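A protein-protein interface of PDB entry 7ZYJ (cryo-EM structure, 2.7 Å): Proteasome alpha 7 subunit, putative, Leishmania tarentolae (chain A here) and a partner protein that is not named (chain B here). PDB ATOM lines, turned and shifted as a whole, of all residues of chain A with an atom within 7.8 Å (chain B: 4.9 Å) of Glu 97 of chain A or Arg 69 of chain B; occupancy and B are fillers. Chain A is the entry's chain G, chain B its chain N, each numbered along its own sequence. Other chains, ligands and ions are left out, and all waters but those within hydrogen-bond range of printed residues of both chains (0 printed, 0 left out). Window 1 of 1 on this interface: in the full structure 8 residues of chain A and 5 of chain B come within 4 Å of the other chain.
The side-chain carboxylate (OE1) of Glu 97 of chain A lies within salt-bridge range of the guanidinium group (NE) of Arg 69 of chain B (3.7 Å). OD1 of Asp 101 of chain A lies within salt-bridge range of NH2 of Arg 69 of chain B (2.9 Å). O of Tyr 73 of chain B sits at hydrogen-bond distance from NH2 of Arg 93 of chain A. The side-chain carboxylate (OE1) of Glu 97 of chain A sits at hydrogen-bond distance from the side-chain hydroxyl (OH) of Tyr 73 of chain B, 2.7 Å away. The backbone carbonyl oxygen of Asp 71 of chain A lies close to the side-chain sulfur of Met 72 of chain B (3.4 Å).
The guanidinium group of Arg 69 of chain B lies within salt-bridge range of the side-chain carboxylate of Asp 65 of chain B (3.4 Å). O of Ala 69 of chain A is in hydrogen-bond range of NE of Arg 93 of chain A (3.0 Å). OD1 of Asp 71 of chain A lies within salt-bridge range of NE of Arg 100 of chain A, at 3.1 Å.
Among the printed residues, merely in contact across the chains: Asp 101 of chain A with Asp 65 of chain B (3.5 Å), Val 70 of chain A with Tyr 73 of chain B (3.8 Å) and Ala 69 of chain A with Met 72 of chain B (3.997 Å).
Printed residues of chain B within 4 Å of Glu 97 of chain A: Arg 69 (3.4 Å) and Tyr 73 (2.7 Å). Arg 69 of chain B touches just these residues of chain A: Glu 97 and Asp 101. Printed residues of chain B within 4 Å of Arg 93 of chain A: Tyr 73 (3.1 Å). Of the printed residues of chain B, Ala 69 of chain A touches Met 72 (3.997 Å). Ser 90 of chain A touches none of the printed residues of chain B. Arg 91 of chain A touches none of the printed residues of chain B. The nearest printed residue of chain B that does not touch Glu 97 of chain A is Asp 65 of chain B (6.3 Å).
Of the 21 printed residues of chain A, 6 touch a printed residue of chain B. Along chain B the printed residues that touch a printed residue of chain A span positions 65 to 73.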
ATOM      1  N   ALA A  69       6.206  12.161 -18.350  1.00  0.00           N
ATOM      2  CA  ALA A  69       7.062  11.867 -19.487  1.00  0.00           C
ATOM      3  C   ALA A  69       6.302  12.114 -20.783  1.00  0.00           C
ATOM      4  O   ALA A  69       5.190  11.608 -20.968  1.00  0.00           O
ATOM      5  CB  ALA A  69       7.555  10.422 -19.426  1.00  0.00           C
ATOM      6  N   VAL A  70       6.900  12.893 -21.674  1.00  0.00           N
ATOM      7  CA  VAL A  70       6.330  13.172 -22.987  1.00  0.00           C
ATOM      8  C   VAL A  70       6.876  12.217 -24.036  1.00  0.00           C
ATOM      9  O   VAL A  70       6.125  11.658 -24.835  1.00  0.00           O
ATOM     10  CB  VAL A  70       6.590  14.644 -23.374  1.00  0.00           C
ATOM     11  CG1 VAL A  70       6.345  14.858 -24.857  1.00  0.00           C
ATOM     12  CG2 VAL A  70       5.719  15.569 -22.544  1.00  0.00           C
ATOM     13  N   ASP A  71       8.191  12.018 -24.037  1.00  0.00           N
ATOM     14  CA  ASP A  71       8.830  11.012 -24.871  1.00  0.00           C
ATOM     15  C   ASP A  71       9.773  10.197 -23.997  1.00  0.00           C
ATOM     16  O   ASP A  71       9.742  10.324 -22.769  1.00  0.00           O
ATOM     17  CB  ASP A  71       9.577  11.663 -26.035  1.00  0.00           C
ATOM     18  CG  ASP A  71       9.659  10.763 -27.252  1.00  0.00           C
ATOM     19  OD1 ASP A  71       9.367   9.556 -27.120  1.00  0.00           O
ATOM     20  OD2 ASP A  71      10.013  11.263 -28.339  1.00  0.00           O
ATOM     21  N   SER A  90      -0.595  16.195 -23.084  1.00  0.00           N
ATOM     22  CA  SER A  90      -1.156  15.382 -24.159  1.00  0.00           C
ATOM     23  C   SER A  90      -0.764  15.932 -25.525  1.00  0.00           C
ATOM     24  O   SER A  90      -0.401  15.172 -26.431  1.00  0.00           O
ATOM     25  CB  SER A  90      -2.676  15.310 -24.025  1.00  0.00           C
ATOM     26  OG  SER A  90      -3.051  14.547 -22.893  1.00  0.00           O
ATOM     27  N   ARG A  91      -0.823  17.256 -25.688  1.00  0.00           N
ATOM     28  CA  ARG A  91      -0.393  17.859 -26.949  1.00  0.00           C
ATOM     29  C   ARG A  91       1.086  17.599 -27.213  1.00  0.00           C
ATOM     30  O   ARG A  91       1.482  17.304 -28.347  1.00  0.00           O
ATOM     31  CB  ARG A  91      -0.678  19.359 -26.941  1.00  0.00           C
ATOM     32  CG  ARG A  91      -0.293  20.064 -28.231  1.00  0.00           C
ATOM     33  CD  ARG A  91      -0.849  19.351 -29.448  1.00  0.00           C
ATOM     34  NE  ARG A  91      -0.602  20.100 -30.674  1.00  0.00           N
ATOM     35  CZ  ARG A  91      -1.552  20.613 -31.443  1.00  0.00           C
ATOM     36  NH1 ARG A  91      -2.833  20.479 -31.139  1.00  0.00           N
ATOM     37  NH2 ARG A  91      -1.210  21.276 -32.542  1.00  0.00           N
ATOM     38  N   ALA A  92       1.920  17.716 -26.179  1.00  0.00           N
ATOM     39  CA  ALA A  92       3.349  17.473 -26.345  1.00  0.00           C
ATOM     40  C   ALA A  92       3.626  16.017 -26.697  1.00  0.00           C
ATOM     41  O   ALA A  92       4.517  15.728 -27.501  1.00  0.00           O
ATOM     42  CB  ALA A  92       4.099  17.869 -25.076  1.00  0.00           C
ATOM     43  N   ARG A  93       2.888  15.089 -26.090  1.00  0.00           N
ATOM     44  CA  ARG A  93       3.033  13.678 -26.429  1.00  0.00           C
ATOM     45  C   ARG A  93       2.616  13.419 -27.870  1.00  0.00           C
ATOM     46  O   ARG A  93       3.241  12.612 -28.566  1.00  0.00           O
ATOM     47  CB  ARG A  93       2.210  12.821 -25.469  1.00  0.00           C
ATOM     48  CG  ARG A  93       2.754  12.783 -24.057  1.00  0.00           C
ATOM     49  CD  ARG A  93       1.717  12.257 -23.087  1.00  0.00           C
ATOM     50  NE  ARG A  93       2.288  11.978 -21.776  1.00  0.00           N
ATOM     51  CZ  ARG A  93       1.608  11.475 -20.756  1.00  0.00           C
ATOM     52  NH1 ARG A  93       0.322  11.187 -20.858  1.00  0.00           N
ATOM     53  NH2 ARG A  93       2.235  11.257 -19.603  1.00  0.00           N
ATOM     54  N   GLN A  94       1.558  14.090 -28.328  1.00  0.00           N
ATOM     55  CA  GLN A  94       1.171  13.985 -29.730  1.00  0.00           C
ATOM     56  C   GLN A  94       2.267  14.513 -30.646  1.00  0.00           C
ATOM     57  O   GLN A  94       2.548  13.923 -31.695  1.00  0.00           O
ATOM     58  CB  GLN A  94      -0.133  14.742 -29.970  1.00  0.00           C
ATOM     59  CG  GLN A  94      -0.772  14.464 -31.316  1.00  0.00           C
ATOM     60  CD  GLN A  94      -1.624  15.618 -31.803  1.00  0.00           C
ATOM     61  OE1 GLN A  94      -1.125  16.544 -32.442  1.00  0.00           O
ATOM     62  NE2 GLN A  94      -2.915  15.571 -31.497  1.00  0.00           N
ATOM     63  N   GLU A  95       2.890  15.631 -30.267  1.00  0.00           N
ATOM     64  CA  GLU A  95       3.973  16.191 -31.070  1.00  0.00           C
ATOM     65  C   GLU A  95       5.181  15.262 -31.105  1.00  0.00           C
ATOM     66  O   GLU A  95       5.827  15.113 -32.149  1.00  0.00           O
ATOM     67  CB  GLU A  95       4.374  17.563 -30.527  1.00  0.00           C
ATOM     68  CG  GLU A  95       3.327  18.643 -30.725  1.00  0.00           C
ATOM     69  CD  GLU A  95       2.979  18.858 -32.183  1.00  0.00           C
ATOM     70  OE1 GLU A  95       3.895  18.806 -33.028  1.00  0.00           O
ATOM     71  OE2 GLU A  95       1.787  19.080 -32.483  1.00  0.00           O
ATOM     72  N   ALA A  96       5.508  14.640 -29.971  1.00  0.00           N
ATOM     73  CA  ALA A  96       6.683  13.779 -29.902  1.00  0.00           C
ATOM     74  C   ALA A  96       6.506  12.507 -30.720  1.00  0.00           C
ATOM     75  O   ALA A  96       7.446  12.070 -31.392  1.00  0.00           O
ATOM     76  CB  ALA A  96       6.998  13.434 -28.448  1.00  0.00           C
ATOM     77  N   GLU A  97       5.321  11.900 -30.680  1.00  0.00           N
ATOM     78  CA  GLU A  97       5.079  10.687 -31.449  1.00  0.00           C
ATOM     79  C   GLU A  97       4.895  10.957 -32.933  1.00  0.00           C
ATOM     80  O   GLU A  97       5.137  10.059 -33.745  1.00  0.00           O
ATOM     81  CB  GLU A  97       3.851   9.946 -30.908  1.00  0.00           C
ATOM     82  CG  GLU A  97       2.550  10.708 -31.034  1.00  0.00           C
ATOM     83  CD  GLU A  97       1.457  10.135 -30.156  1.00  0.00           C
ATOM     84  OE1 GLU A  97       1.780   9.610 -29.070  1.00  0.00           O
ATOM     85  OE2 GLU A  97       0.275  10.209 -30.550  1.00  0.00           O
ATOM     86  N   ASN A  98       4.474  12.168 -33.306  1.00  0.00           N
ATOM     87  CA  ASN A  98       4.423  12.529 -34.717  1.00  0.00           C
ATOM     88  C   ASN A  98       5.816  12.527 -35.330  1.00  0.00           C
ATOM     89  O   ASN A  98       6.003  12.068 -36.462  1.00  0.00           O
ATOM     90  CB  ASN A  98       3.765  13.897 -34.886  1.00  0.00           C
ATOM     91  CG  ASN A  98       2.271  13.800 -35.116  1.00  0.00           C
ATOM     92  OD1 ASN A  98       1.676  12.732 -34.978  1.00  0.00           O
ATOM     93  ND2 ASN A  98       1.653  14.923 -35.464  1.00  0.00           N
ATOM     94  N   SER A  99       6.804  13.044 -34.598  1.00  0.00           N
ATOM     95  CA  SER A  99       8.179  13.029 -35.085  1.00  0.00           C
ATOM     96  C   SER A  99       8.701  11.605 -35.217  1.00  0.00           C
ATOM     97  O   SER A  99       9.403  11.278 -36.182  1.00  0.00           O
ATOM     98  CB  SER A  99       9.070  13.848 -34.153  1.00  0.00           C
ATOM     99  OG  SER A  99      10.409  13.872 -34.612  1.00  0.00           O
ATOM    100  N   ARG A 100       8.368  10.742 -34.257  1.00  0.00           N
ATOM    101  CA  ARG A 100       8.849   9.366 -34.283  1.00  0.00           C
ATOM    102  C   ARG A 100       8.140   8.522 -35.333  1.00  0.00           C
ATOM    103  O   ARG A 100       8.645   7.454 -35.694  1.00  0.00           O
ATOM    104  CB  ARG A 100       8.676   8.733 -32.904  1.00  0.00           C
ATOM    105  CG  ARG A 100       9.897   8.841 -32.015  1.00  0.00           C
ATOM    106  CD  ARG A 100       9.793   7.906 -30.829  1.00  0.00           C
ATOM    107  NE  ARG A 100      10.575   8.376 -29.693  1.00  0.00           N
ATOM    108  CZ  ARG A 100      11.876   8.169 -29.544  1.00  0.00           C
ATOM    109  NH1 ARG A 100      12.575   7.495 -30.441  1.00  0.00           N
ATOM    110  NH2 ARG A 100      12.489   8.647 -28.465  1.00  0.00           N
ATOM    111  N   ASP A 101       6.991   8.971 -35.830  1.00  0.00           N
ATOM    112  CA  ASP A 101       6.213   8.230 -36.815  1.00  0.00           C
ATOM    113  C   ASP A 101       6.324   8.791 -38.222  1.00  0.00           C
ATOM    114  O   ASP A 101       6.308   8.026 -39.188  1.00  0.00           O
ATOM    115  CB  ASP A 101       4.737   8.197 -36.405  1.00  0.00           C
ATOM    116  CG  ASP A 101       4.505   7.408 -35.133  1.00  0.00           C
ATOM    117  OD1 ASP A 101       5.497   7.027 -34.480  1.00  0.00           O
ATOM    118  OD2 ASP A 101       3.329   7.171 -34.785  1.00  0.00           O
ATOM    119  N   ILE A 102       6.434  10.108 -38.364  1.00  0.00           N
ATOM    120  CA  ILE A 102       6.530  10.719 -39.686  1.00  0.00           C
ATOM    121  C   ILE A 102       7.981  10.908 -40.108  1.00  0.00           C
ATOM    122  O   ILE A 102       8.315  10.763 -41.286  1.00  0.00           O
ATOM    123  CB  ILE A 102       5.757  12.053 -39.703  1.00  0.00           C
ATOM    124  CG1 ILE A 102       4.306  11.830 -39.279  1.00  0.00           C
ATOM    125  CG2 ILE A 102       5.818  12.698 -41.079  1.00  0.00           C
ATOM    126  CD1 ILE A 102       3.434  11.238 -40.362  1.00  0.00           C
ATOM    127  N   PHE A 103       8.866  11.217 -39.162  1.00  0.00           N
ATOM    128  CA  PHE A 103      10.256  11.511 -39.471  1.00  0.00           C
ATOM    129  C   PHE A 103      11.229  10.496 -38.892  1.00  0.00           C
ATOM    130  O   PHE A 103      12.435  10.612 -39.132  1.00  0.00           O
ATOM    131  CB  PHE A 103      10.610  12.918 -38.980  1.00  0.00           C
ATOM    132  CG  PHE A 103       9.776  13.997 -39.605  1.00  0.00           C
ATOM    133  CD1 PHE A 103       9.968  14.360 -40.927  1.00  0.00           C
ATOM    134  CD2 PHE A 103       8.790  14.639 -38.877  1.00  0.00           C
ATOM    135  CE1 PHE A 103       9.199  15.346 -41.507  1.00  0.00           C
ATOM    136  CE2 PHE A 103       8.017  15.627 -39.453  1.00  0.00           C
ATOM    137  CZ  PHE A 103       8.223  15.981 -40.769  1.00  0.00           C
ATOM    138  N   ALA A 104      10.739   9.505 -38.147  1.00  0.00           N
ATOM    139  CA  ALA A 104      11.557   8.403 -37.637  1.00  0.00           C
ATOM    140  C   ALA A 104      12.764   8.913 -36.853  1.00  0.00           C
ATOM    141  O   ALA A 104      13.890   8.436 -37.012  1.00  0.00           O
ATOM    142  CB  ALA A 104      11.994   7.479 -38.774  1.00  0.00           C
ATOM    143  N   THR A 105      12.521   9.903 -35.993  1.00  0.00           N
ATOM    144  CA  THR A 105      13.576  10.465 -35.168  1.00  0.00           C
ATOM    145  C   THR A 105      12.969  11.031 -33.896  1.00  0.00           C
ATOM    146  O   THR A 105      11.839  11.540 -33.931  1.00  0.00           O
ATOM    147  CB  THR A 105      14.361  11.557 -35.908  1.00  0.00           C
ATOM    148  OG1 THR A 105      15.387  12.080 -35.055  1.00  0.00           O
ATOM    149  CG2 THR A 105      13.443  12.688 -36.350  1.00  0.00           C
ATOM    150  N   ILE A 107      12.123  13.728 -31.137  1.00  0.00           N
ATOM    151  CA  ILE A 107      11.934  15.162 -31.305  1.00  0.00           C
ATOM    152  C   ILE A 107      12.994  15.911 -30.508  1.00  0.00           C
ATOM    153  O   ILE A 107      13.284  15.577 -29.352  1.00  0.00           O
ATOM    154  CB  ILE A 107      10.507  15.572 -30.901  1.00  0.00           C
ATOM    155  CG1 ILE A 107      10.232  17.023 -31.301  1.00  0.00           C
ATOM    156  CG2 ILE A 107      10.256  15.343 -29.414  1.00  0.00           C
ATOM    157  CD1 ILE A 107       8.775  17.410 -31.211  1.00  0.00           C
ATOM    158  N   LEU A 112      10.399  20.537 -29.639  1.00  0.00           N
ATOM    159  CA  LEU A 112       9.269  20.249 -28.762  1.00  0.00           C
ATOM    160  C   LEU A 112       8.836  21.490 -27.992  1.00  0.00           C
ATOM    161  O   LEU A 112       7.636  21.745 -27.832  1.00  0.00           O
ATOM    162  CB  LEU A 112       9.629  19.118 -27.800  1.00  0.00           C
ATOM    163  CG  LEU A 112       8.592  18.795 -26.725  1.00  0.00           C
ATOM    164  CD1 LEU A 112       7.351  18.182 -27.348  1.00  0.00           C
ATOM    165  CD2 LEU A 112       9.181  17.872 -25.675  1.00  0.00           C
ATOM    166  N   ASP B  65       4.307   0.779 -30.904  1.00  0.00           N
ATOM    167  CA  ASP B  65       3.984   2.117 -30.421  1.00  0.00           C
ATOM    168  C   ASP B  65       2.897   2.077 -29.356  1.00  0.00           C
ATOM    169  O   ASP B  65       2.954   2.835 -28.382  1.00  0.00           O
ATOM    170  CB  ASP B  65       3.553   3.010 -31.584  1.00  0.00           C
ATOM    171  CG  ASP B  65       4.679   3.274 -32.563  1.00  0.00           C
ATOM    172  OD1 ASP B  65       5.842   2.965 -32.231  1.00  0.00           O
ATOM    173  OD2 ASP B  65       4.400   3.789 -33.665  1.00  0.00           O
ATOM    174  N   ASN B  66       1.904   1.202 -29.525  1.00  0.00           N
ATOM    175  CA  ASN B  66       0.808   1.116 -28.566  1.00  0.00           C
ATOM    176  C   ASN B  66       1.281   0.662 -27.191  1.00  0.00           C
ATOM    177  O   ASN B  66       0.815   1.189 -26.175  1.00  0.00           O
ATOM    178  CB  ASN B  66      -0.268   0.169 -29.097  1.00  0.00           C
ATOM    179  CG  ASN B  66      -1.519   0.171 -28.245  1.00  0.00           C
ATOM    180  OD1 ASN B  66      -1.740  -0.738 -27.446  1.00  0.00           O
ATOM    181  ND2 ASN B  66      -2.349   1.193 -28.414  1.00  0.00           N
ATOM    182  N   ILE B  67       2.192  -0.311 -27.133  1.00  0.00           N
ATOM    183  CA  ILE B  67       2.659  -0.821 -25.846  1.00  0.00           C
ATOM    184  C   ILE B  67       3.473   0.239 -25.114  1.00  0.00           C
ATOM    185  O   ILE B  67       3.217   0.546 -23.941  1.00  0.00           O
ATOM    186  CB  ILE B  67       3.479  -2.107 -26.048  1.00  0.00           C
ATOM    187  CG1 ILE B  67       2.644  -3.179 -26.746  1.00  0.00           C
ATOM    188  CG2 ILE B  67       4.003  -2.622 -24.717  1.00  0.00           C
ATOM    189  CD1 ILE B  67       3.448  -4.389 -27.156  1.00  0.00           C
ATOM    190  N   GLU B  68       4.465   0.813 -25.797  1.00  0.00           N
ATOM    191  CA  GLU B  68       5.376   1.748 -25.149  1.00  0.00           C
ATOM    192  C   GLU B  68       4.652   3.013 -24.710  1.00  0.00           C
ATOM    193  O   GLU B  68       4.897   3.527 -23.613  1.00  0.00           O
ATOM    194  CB  GLU B  68       6.531   2.090 -26.091  1.00  0.00           C
ATOM    195  CG  GLU B  68       7.631   2.941 -25.471  1.00  0.00           C
ATOM    196  CD  GLU B  68       8.100   2.419 -24.124  1.00  0.00           C
ATOM    197  OE1 GLU B  68       9.005   1.558 -24.104  1.00  0.00           O
ATOM    198  OE2 GLU B  68       7.580   2.878 -23.087  1.00  0.00           O
ATOM    199  N   ARG B  69       3.759   3.532 -25.554  1.00  0.00           N
ATOM    200  CA  ARG B  69       3.039   4.751 -25.203  1.00  0.00           C
ATOM    201  C   ARG B  69       2.108   4.525 -24.019  1.00  0.00           C
ATOM    202  O   ARG B  69       2.004   5.380 -23.134  1.00  0.00           O
ATOM    203  CB  ARG B  69       2.265   5.267 -26.415  1.00  0.00           C
ATOM    204  CG  ARG B  69       3.135   6.016 -27.406  1.00  0.00           C
ATOM    205  CD  ARG B  69       2.480   6.108 -28.769  1.00  0.00           C
ATOM    206  NE  ARG B  69       3.459   6.375 -29.817  1.00  0.00           N
ATOM    207  CZ  ARG B  69       3.160   6.523 -31.100  1.00  0.00           C
ATOM    208  NH1 ARG B  69       1.913   6.443 -31.533  1.00  0.00           N
ATOM    209  NH2 ARG B  69       4.138   6.757 -31.970  1.00  0.00           N
ATOM    210  N   GLN B  70       1.422   3.379 -23.983  1.00  0.00           N
ATOM    211  CA  GLN B  70       0.562   3.077 -22.844  1.00  0.00           C
ATOM    212  C   GLN B  70       1.372   2.921 -21.565  1.00  0.00           C
ATOM    213  O   GLN B  70       0.962   3.398 -20.500  1.00  0.00           O
ATOM    214  CB  GLN B  70      -0.256   1.815 -23.112  1.00  0.00           C
ATOM    215  CG  GLN B  70      -1.238   1.490 -22.000  1.00  0.00           C
ATOM    216  CD  GLN B  70      -2.083   0.273 -22.302  1.00  0.00           C
ATOM    217  OE1 GLN B  70      -1.918  -0.368 -23.339  1.00  0.00           O
ATOM    218  NE2 GLN B  70      -2.991  -0.056 -21.393  1.00  0.00           N
ATOM    219  N   LYS B  71       2.522   2.246 -21.643  1.00  0.00           N
ATOM    220  CA  LYS B  71       3.362   2.098 -20.460  1.00  0.00           C
ATOM    221  C   LYS B  71       3.915   3.438 -19.987  1.00  0.00           C
ATOM    222  O   LYS B  71       4.025   3.671 -18.779  1.00  0.00           O
ATOM    223  CB  LYS B  71       4.505   1.125 -20.745  1.00  0.00           C
ATOM    224  CG  LYS B  71       5.415   0.871 -19.555  1.00  0.00           C
ATOM    225  CD  LYS B  71       6.448  -0.199 -19.863  1.00  0.00           C
ATOM    226  CE  LYS B  71       7.518   0.324 -20.805  1.00  0.00           C
ATOM    227  NZ  LYS B  71       8.601  -0.672 -21.027  1.00  0.00           N
ATOM    228  N   MET B  72       4.260   4.326 -20.919  1.00  0.00           N
ATOM    229  CA  MET B  72       4.902   5.595 -20.599  1.00  0.00           C
ATOM    230  C   MET B  72       3.915   6.670 -20.161  1.00  0.00           C
ATOM    231  O   MET B  72       4.199   7.423 -19.223  1.00  0.00           O
ATOM    232  CB  MET B  72       5.693   6.093 -21.811  1.00  0.00           C
ATOM    233  CG  MET B  72       6.795   7.078 -21.479  1.00  0.00           C
ATOM    234  SD  MET B  72       7.068   8.259 -22.814  1.00  0.00           S
ATOM    235  CE  MET B  72       7.428   7.152 -24.174  1.00  0.00           C
ATOM    236  N   TYR B  73       2.760   6.762 -20.822  1.00  0.00           N
ATOM    237  CA  TYR B  73       1.831   7.853 -20.544  1.00  0.00           C
ATOM    238  C   TYR B  73       1.122   7.671 -19.208  1.00  0.00           C
ATOM    239  O   TYR B  73       0.843   8.656 -18.515  1.00  0.00           O
ATOM    240  CB  TYR B  73       0.810   7.977 -21.676  1.00  0.00           C
ATOM    241  CG  TYR B  73       1.391   8.414 -23.002  1.00  0.00           C
ATOM    242  CD1 TYR B  73       2.721   8.798 -23.114  1.00  0.00           C
ATOM    243  CD2 TYR B  73       0.607   8.440 -24.147  1.00  0.00           C
ATOM    244  CE1 TYR B  73       3.252   9.194 -24.324  1.00  0.00           C
ATOM    245  CE2 TYR B  73       1.129   8.835 -25.361  1.00  0.00           C
ATOM    246  CZ  TYR B  73       2.451   9.211 -25.445  1.00  0.00           C
ATOM    247  OH  TYR B  73       2.975   9.606 -26.653  1.00  0.00           O
ATOM    248  N   HIS B  74       0.822   6.434 -18.831  1.00  0.00           N
ATOM    249  CA  HIS B  74       0.127   6.143 -17.588  1.00  0.00           C
ATOM    250  C   HIS B  74       0.950   5.192 -16.732  1.00  0.00           C
ATOM    251  O   HIS B  74       1.678   4.338 -17.245  1.00  0.00           O
ATOM    252  CB  HIS B  74      -1.253   5.537 -17.857  1.00  0.00           C
ATOM    253  CG  HIS B  74      -1.912   6.062 -19.093  1.00  0.00           C
ATOM    254  ND1 HIS B  74      -2.522   7.297 -19.144  1.00  0.00           N
ATOM    255  CD2 HIS B  74      -2.054   5.522 -20.326  1.00  0.00           C
ATOM    256  CE1 HIS B  74      -3.012   7.494 -20.354  1.00  0.00           C
ATOM    257  NE2 HIS B  74      -2.742   6.432 -21.091  1.00  0.00           N
